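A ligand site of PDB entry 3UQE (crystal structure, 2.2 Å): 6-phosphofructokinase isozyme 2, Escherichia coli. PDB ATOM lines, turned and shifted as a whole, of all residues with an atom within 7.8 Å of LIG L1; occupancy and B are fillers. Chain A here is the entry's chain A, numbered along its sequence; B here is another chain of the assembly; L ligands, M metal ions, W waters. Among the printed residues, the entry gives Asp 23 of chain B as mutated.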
ATOM      1  N   ARG A 105     -25.024   4.849   6.140  1.00  0.00           N
ATOM      2  CA  ARG A 105     -24.426   4.481   4.867  1.00  0.00           C
ATOM      3  C   ARG A 105     -25.495   4.342   3.804  1.00  0.00           C
ATOM      4  O   ARG A 105     -26.328   3.443   3.880  1.00  0.00           O
ATOM      5  CB  ARG A 105     -23.645   3.175   4.987  1.00  0.00           C
ATOM      6  CG  ARG A 105     -22.488   3.241   5.978  1.00  0.00           C
ATOM      7  CD  ARG A 105     -22.364   1.951   6.780  1.00  0.00           C
ATOM      8  NE  ARG A 105     -21.741   0.879   6.011  1.00  0.00           N
ATOM      9  CZ  ARG A 105     -21.720  -0.401   6.387  1.00  0.00           C
ATOM     10  NH1 ARG A 105     -22.292  -0.769   7.530  1.00  0.00           N
ATOM     11  NH2 ARG A 105     -21.112  -1.302   5.630  1.00  0.00           N
ATOM     12  N   SER A 167     -21.139 -12.437  -2.364  1.00  0.00           N
ATOM     13  CA  SER A 167     -22.141 -11.639  -3.029  1.00  0.00           C
ATOM     14  C   SER A 167     -23.477 -11.883  -2.362  1.00  0.00           C
ATOM     15  O   SER A 167     -23.533 -12.345  -1.221  1.00  0.00           O
ATOM     16  CB  SER A 167     -22.214 -11.997  -4.515  1.00  0.00           C
ATOM     17  OG  SER A 167     -23.111 -11.153  -5.196  1.00  0.00           O
ATOM     18  N   SER A 168     -24.561 -11.555  -3.065  1.00  0.00           N
ATOM     19  CA  SER A 168     -25.903 -11.731  -2.518  1.00  0.00           C
ATOM     20  C   SER A 168     -26.937 -11.750  -3.630  1.00  0.00           C
ATOM     21  O   SER A 168     -26.603 -11.594  -4.805  1.00  0.00           O
ATOM     22  CB  SER A 168     -26.239 -10.616  -1.540  1.00  0.00           C
ATOM     23  OG  SER A 168     -26.358  -9.371  -2.204  1.00  0.00           O
ATOM     24  N   LYS A 185     -18.594 -16.835   1.355  1.00  0.00           N
ATOM     25  CA  LYS A 185     -18.915 -16.325   2.690  1.00  0.00           C
ATOM     26  C   LYS A 185     -20.229 -15.577   2.702  1.00  0.00           C
ATOM     27  O   LYS A 185     -20.245 -14.352   2.553  1.00  0.00           O
ATOM     28  CB  LYS A 185     -17.802 -15.432   3.265  1.00  0.00           C
ATOM     29  CG  LYS A 185     -18.085 -14.993   4.699  1.00  0.00           C
ATOM     30  CD  LYS A 185     -17.603 -13.567   5.002  1.00  0.00           C
ATOM     31  CE  LYS A 185     -18.528 -12.510   4.411  1.00  0.00           C
ATOM     32  NZ  LYS A 185     -19.980 -12.752   4.700  1.00  0.00           N
ATOM     33  N   ASN A 187     -23.419 -14.142   4.814  1.00  0.00           N
ATOM     34  CA  ASN A 187     -23.870 -13.927   6.189  1.00  0.00           C
ATOM     35  C   ASN A 187     -25.178 -14.678   6.374  1.00  0.00           C
ATOM     36  O   ASN A 187     -25.605 -15.394   5.468  1.00  0.00           O
ATOM     37  CB  ASN A 187     -24.013 -12.433   6.515  1.00  0.00           C
ATOM     38  CG  ASN A 187     -25.042 -11.717   5.650  1.00  0.00           C
ATOM     39  OD1 ASN A 187     -25.823 -12.358   4.934  1.00  0.00           O
ATOM     40  ND2 ASN A 187     -25.048 -10.386   5.701  1.00  0.00           N
ATOM     41  N   GLN A 188     -25.813 -14.519   7.527  1.00  0.00           N
ATOM     42  CA  GLN A 188     -27.048 -15.230   7.829  1.00  0.00           C
ATOM     43  C   GLN A 188     -28.184 -14.893   6.850  1.00  0.00           C
ATOM     44  O   GLN A 188     -28.933 -15.776   6.429  1.00  0.00           O
ATOM     45  CB  GLN A 188     -27.481 -14.954   9.278  1.00  0.00           C
ATOM     46  CG  GLN A 188     -28.990 -14.909   9.504  1.00  0.00           C
ATOM     47  CD  GLN A 188     -29.610 -16.278   9.741  1.00  0.00           C
ATOM     48  OE1 GLN A 188     -30.228 -16.858   8.833  1.00  0.00           O
ATOM     49  NE2 GLN A 188     -29.468 -16.798  10.958  1.00  0.00           N
ATOM     50  N   LYS A 189     -28.304 -13.621   6.482  1.00  0.00           N
ATOM     51  CA  LYS A 189     -29.312 -13.171   5.530  1.00  0.00           C
ATOM     52  C   LYS A 189     -29.083 -13.781   4.143  1.00  0.00           C
ATOM     53  O   LYS A 189     -30.002 -14.286   3.508  1.00  0.00           O
ATOM     54  CB  LYS A 189     -29.313 -11.644   5.439  1.00  0.00           C
ATOM     55  CG  LYS A 189     -30.467 -11.062   4.645  1.00  0.00           C
ATOM     56  CD  LYS A 189     -30.631  -9.571   4.925  1.00  0.00           C
ATOM     57  CE  LYS A 189     -29.891  -8.709   3.915  1.00  0.00           C
ATOM     58  NZ  LYS A 189     -29.597  -7.349   4.454  1.00  0.00           N
ATOM     59  N   GLU A 190     -27.831 -13.739   3.695  1.00  0.00           N
ATOM     60  CA  GLU A 190     -27.465 -14.254   2.379  1.00  0.00           C
ATOM     61  C   GLU A 190     -27.596 -15.777   2.271  1.00  0.00           C
ATOM     62  O   GLU A 190     -27.964 -16.296   1.226  1.00  0.00           O
ATOM     63  CB  GLU A 190     -26.059 -13.778   2.005  1.00  0.00           C
ATOM     64  CG  GLU A 190     -25.977 -12.269   1.774  1.00  0.00           C
ATOM     65  CD  GLU A 190     -24.563 -11.721   1.899  1.00  0.00           C
ATOM     66  OE1 GLU A 190     -24.363 -10.531   1.577  1.00  0.00           O
ATOM     67  OE2 GLU A 190     -23.659 -12.478   2.322  1.00  0.00           O
ATOM     68  N   SER A 224     -20.850 -16.200   8.043  1.00  0.00           N
ATOM     69  CA  SER A 224     -20.491 -15.203   9.028  1.00  0.00           C
ATOM     70  C   SER A 224     -21.742 -14.816   9.809  1.00  0.00           C
ATOM     71  O   SER A 224     -22.827 -14.682   9.240  1.00  0.00           O
ATOM     72  CB  SER A 224     -19.800 -13.983   8.374  1.00  0.00           C
ATOM     73  OG  SER A 224     -20.607 -13.395   7.379  1.00  0.00           O
ATOM     74  N   THR A 251     -19.342  -1.653  12.099  1.00  0.00           N
ATOM     75  CA  THR A 251     -19.501  -2.923  11.400  1.00  0.00           C
ATOM     76  C   THR A 251     -18.838  -2.846  10.035  1.00  0.00           C
ATOM     77  O   THR A 251     -18.685  -3.853   9.350  1.00  0.00           O
ATOM     78  CB  THR A 251     -20.976  -3.331  11.244  1.00  0.00           C
ATOM     79  OG1 THR A 251     -21.713  -2.254  10.645  1.00  0.00           O
ATOM     80  CG2 THR A 251     -21.584  -3.661  12.601  1.00  0.00           C
ATOM     81  N   VAL A 252     -18.442  -1.644   9.660  1.00  0.00           N
ATOM     82  CA  VAL A 252     -17.714  -1.413   8.410  1.00  0.00           C
ATOM     83  C   VAL A 252     -16.231  -1.702   8.625  1.00  0.00           C
ATOM     84  O   VAL A 252     -15.672  -1.307   9.641  1.00  0.00           O
ATOM     85  CB  VAL A 252     -17.805   0.073   8.009  1.00  0.00           C
ATOM     86  CG1 VAL A 252     -17.532   0.256   6.514  1.00  0.00           C
ATOM     87  CG2 VAL A 252     -19.162   0.638   8.404  1.00  0.00           C
ATOM     88  N   GLY A 255     -17.065  -7.779   6.697  1.00  0.00           N
ATOM     89  CA  GLY A 255     -17.181  -8.901   5.789  1.00  0.00           C
ATOM     90  C   GLY A 255     -15.980  -8.996   4.869  1.00  0.00           C
ATOM     91  O   GLY A 255     -15.404 -10.070   4.711  1.00  0.00           O
ATOM     92  N   ASP B  23     -31.839   4.000   9.296  1.00  0.00           N
ATOM     93  CA  ASP B  23     -31.351   3.524  10.578  1.00  0.00           C
ATOM     94  C   ASP B  23     -29.831   3.512  10.564  1.00  0.00           C
ATOM     95  O   ASP B  23     -29.223   3.361   9.503  1.00  0.00           O
ATOM     96  CB  ASP B  23     -31.911   2.124  10.880  1.00  0.00           C
ATOM     97  CG  ASP B  23     -31.777   1.172   9.707  1.00  0.00           C
ATOM     98  OD1 ASP B  23     -30.638   0.749   9.402  1.00  0.00           O
ATOM     99  OD2 ASP B  23     -32.815   0.840   9.092  1.00  0.00           O
ATOM    100  N   PRO B  24     -29.194   3.659  11.735  1.00  0.00           N
ATOM    101  CA  PRO B  24     -27.738   3.762  11.761  1.00  0.00           C
ATOM    102  C   PRO B  24     -27.074   2.408  11.533  1.00  0.00           C
ATOM    103  O   PRO B  24     -27.763   1.388  11.502  1.00  0.00           O
ATOM    104  CB  PRO B  24     -27.448   4.220  13.199  1.00  0.00           C
ATOM    105  CG  PRO B  24     -28.796   4.477  13.846  1.00  0.00           C
ATOM    106  CD  PRO B  24     -29.775   3.663  13.084  1.00  0.00           C
ATOM    107  N   GLU B  25     -25.756   2.413  11.370  1.00  0.00           N
ATOM    108  CA  GLU B  25     -24.917   1.194  11.361  1.00  0.00           C
ATOM    109  C   GLU B  25     -24.984   0.346  10.090  1.00  0.00           C
ATOM    110  O   GLU B  25     -23.965   0.176   9.405  1.00  0.00           O
ATOM    111  CB  GLU B  25     -25.184   0.333  12.597  1.00  0.00           C
ATOM    112  N   GLY B  26     -26.155  -0.195   9.773  1.00  0.00           N
ATOM    113  CA  GLY B  26     -26.297  -1.082   8.627  1.00  0.00           C
ATOM    114  C   GLY B  26     -26.140  -0.382   7.287  1.00  0.00           C
ATOM    115  O   GLY B  26     -25.943   0.832   7.225  1.00  0.00           O
ATOM    116  N   LYS B  27     -26.204  -1.166   6.211  1.00  0.00           N
ATOM    117  CA  LYS B  27     -26.190  -0.613   4.859  1.00  0.00           C
ATOM    118  C   LYS B  27     -27.608  -0.232   4.440  1.00  0.00           C
ATOM    119  O   LYS B  27     -28.516  -1.062   4.514  1.00  0.00           O
ATOM    120  CB  LYS B  27     -25.639  -1.628   3.855  1.00  0.00           C
ATOM    121  CG  LYS B  27     -24.223  -2.085   4.111  1.00  0.00           C
ATOM    122  CD  LYS B  27     -23.911  -3.287   3.232  1.00  0.00           C
ATOM    123  CE  LYS B  27     -22.636  -3.971   3.694  1.00  0.00           C
ATOM    124  NZ  LYS B  27     -22.578  -5.392   3.236  1.00  0.00           N
ATOM    125  N   LEU B  28     -27.797   0.992   3.977  1.00  0.00           N
ATOM    126  CA  LEU B  28     -29.096   1.416   3.467  1.00  0.00           C
ATOM    127  C   LEU B  28     -29.113   1.327   1.954  1.00  0.00           C
ATOM    128  O   LEU B  28     -28.574   2.187   1.252  1.00  0.00           O
ATOM    129  CB  LEU B  28     -29.436   2.826   3.937  1.00  0.00           C
ATOM    130  CG  LEU B  28     -29.385   2.999   5.458  1.00  0.00           C
ATOM    131  CD1 LEU B  28     -29.730   4.416   5.870  1.00  0.00           C
ATOM    132  CD2 LEU B  28     -30.287   1.986   6.146  1.00  0.00           C
ATOM    133  N   ARG B  29     -29.711   0.256   1.442  1.00  0.00           N
ATOM    134  CA  ARG B  29     -29.781   0.022   0.008  1.00  0.00           C
ATOM    135  C   ARG B  29     -30.678   1.048  -0.672  1.00  0.00           C
ATOM    136  O   ARG B  29     -31.880   1.124  -0.393  1.00  0.00           O
ATOM    137  CB  ARG B  29     -30.260  -1.402  -0.282  1.00  0.00           C
ATOM    138  CG  ARG B  29     -29.281  -2.484   0.155  1.00  0.00           C
ATOM    139  CD  ARG B  29     -29.855  -3.875  -0.032  1.00  0.00           C
ATOM    140  NE  ARG B  29     -30.366  -4.083  -1.382  1.00  0.00           N
ATOM    141  CZ  ARG B  29     -29.623  -4.434  -2.417  1.00  0.00           C
ATOM    142  NH1 ARG B  29     -28.316  -4.626  -2.268  1.00  0.00           N
ATOM    143  NH2 ARG B  29     -30.177  -4.597  -3.611  1.00  0.00           N
HETATM  144  P1  LIG L   1     -25.748  -6.925   4.552  1.00  0.00           P
HETATM  145  O1  LIG L   1     -24.373  -7.428   5.293  1.00  0.00           O
HETATM  146  O2  LIG L   1     -26.833  -8.156   4.494  1.00  0.00           O
HETATM  147  O3  LIG L   1     -25.373  -6.453   3.025  1.00  0.00           O
HETATM  148  O4  LIG L   1     -26.385  -5.594   5.305  1.00  0.00           O
HETATM  149  P2  LIG L   1     -26.454  -5.454   6.931  1.00  0.00           P
HETATM  150  O5  LIG L   1     -25.092  -4.660   7.328  1.00  0.00           O
HETATM  151  O6  LIG L   1     -26.527  -6.928   7.696  1.00  0.00           O
HETATM  152  O7  LIG L   1     -27.800  -4.603   7.387  1.00  0.00           O
HETATM  153  P1  LG2 L   2     -20.527  -6.771   5.728  1.00  0.00           P
HETATM  154  O1  LG2 L   2     -21.965  -6.044   6.078  1.00  0.00           O
HETATM  155  O2  LG2 L   2     -20.560  -7.332   4.185  1.00  0.00           O
HETATM  156  O3  LG2 L   2     -19.444  -5.808   5.873  1.00  0.00           O
HETATM  157  P2  LG2 L   2     -21.144  -9.405   6.614  1.00  0.00           P
HETATM  158  O4  LG2 L   2     -21.009  -9.949   5.075  1.00  0.00           O
HETATM  159  O5  LG2 L   2     -22.541  -9.136   6.919  1.00  0.00           O
HETATM  160  O6  LG2 L   2     -20.278  -8.008   6.781  1.00  0.00           O
HETATM  161  P3  LG2 L   2     -20.468 -10.258   9.285  1.00  0.00           P
HETATM  162  O7  LG2 L   2     -21.503  -9.060   9.735  1.00  0.00           O
HETATM  163  O8  LG2 L   2     -20.816 -11.485   9.997  1.00  0.00           O
HETATM  164  O9  LG2 L   2     -20.551 -10.540   7.656  1.00  0.00           O
HETATM  165  O10 LG2 L   2     -18.927  -9.827   9.664  1.00  0.00           O
HETATM  166  C1  LG2 L   2     -17.858 -10.673   9.318  1.00  0.00           C
HETATM  167  C2  LG2 L   2     -16.995 -10.941  10.558  1.00  0.00           C
HETATM  168  O11 LG2 L   2     -16.630  -9.688  11.200  1.00  0.00           O
HETATM  169  C3  LG2 L   2     -17.779 -11.734  11.603  1.00  0.00           C
HETATM  170  O12 LG2 L   2     -17.689 -13.107  11.371  1.00  0.00           O
HETATM  171  C4  LG2 L   2     -17.073 -11.357  12.868  1.00  0.00           C
HETATM  172  O13 LG2 L   2     -15.900 -12.115  13.028  1.00  0.00           O
HETATM  173  C5  LG2 L   2     -16.706  -9.883  12.647  1.00  0.00           C
HETATM  174  N1  LG2 L   2     -17.790  -9.092  13.210  1.00  0.00           N
HETATM  175  C6  LG2 L   2     -18.922  -8.483  12.458  1.00  0.00           C
HETATM  176  N2  LG2 L   2     -19.771  -7.781  13.417  1.00  0.00           N
HETATM  177  C7  LG2 L   2     -19.180  -7.955  14.752  1.00  0.00           C
HETATM  178  C8  LG2 L   2     -19.607  -7.457  16.112  1.00  0.00           C
HETATM  179  N3  LG2 L   2     -20.804  -6.664  16.253  1.00  0.00           N
HETATM  180  N4  LG2 L   2     -18.807  -7.793  17.289  1.00  0.00           N
HETATM  181  C9  LG2 L   2     -17.560  -8.612  17.141  1.00  0.00           C
HETATM  182  N5  LG2 L   2     -17.139  -9.102  15.803  1.00  0.00           N
HETATM  183  C10 LG2 L   2     -17.947  -8.772  14.621  1.00  0.00           C
HETATM  184 MG    MG M   1     -23.715  -7.021   7.883  1.00  0.00          MG
HETATM  185 MG    MG M   2     -21.014  -9.725   2.572  1.00  0.00          MG
HETATM  186  O   HOH W   1     -27.398  -4.908   1.877  1.00  0.00           O
HETATM  187  O   HOH W   2     -21.732  -4.021   7.791  1.00  0.00           O
HETATM  188  O   HOH W   3     -28.749  -3.745   4.541  1.00  0.00           O
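Gly 26 of chain B touches LIG L1. Four residues have an atom within 4 Å of LIG L1: Asn 187, Lys 189, Gly 26 of chain B and Lys 27 of chain B.
The side-chain amide oxygen of Asn 187 is in hydrogen-bond range of the backbone NH of Lys 189, 3.2 Å away. OD1 of Asn 187 lies within hydrogen-bond range of N of Glu 190 (2.7 Å).
Water W3 lies within hydrogen-bond range of the backbone carbonyl oxygen of Lys 27 of chain B (2.7 Å) and an oxygen (O4) of LIG L1 (3.1 Å). Water W2 lies within hydrogen-bond range of O1 of LG2 L2, NH1 of Arg 105, OG1 of Thr 251 and O5 of LIG L1.
NZ of Lys 189 lies within salt-bridge range of O2 of LIG L1 (2.9 Å). The side-chain amino group (NZ) of Lys 27 of chain B is in salt-bridge range of an oxygen (O3) of LIG L1, at 3.0 Å. The side-chain amide nitrogen of Asn 187 lies within hydrogen-bond range of an oxygen (O1) of LIG L1 (3.1 Å). NZ of Lys 27 of chain B is in salt-bridge range of O2 of LG2 L2 (3.0 Å). O5 of LG2 L2 sits at hydrogen-bond distance from ND2 of Asn 187 (3.1 Å). The side-chain amino group (NZ) of Lys 185 lies close to an oxygen (O4) of LG2 L2. N of Gly 255 is in hydrogen-bond range of O3 of LG2 L2, 3.2 Å away. The side-chain hydroxyl of Ser 224 lies within hydrogen-bond range of an oxygen (O9) of LG2 L2, at 2.9 Å.
O1 of LIG L1 sits close to O1 of LG2 L2 (2.9 Å).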
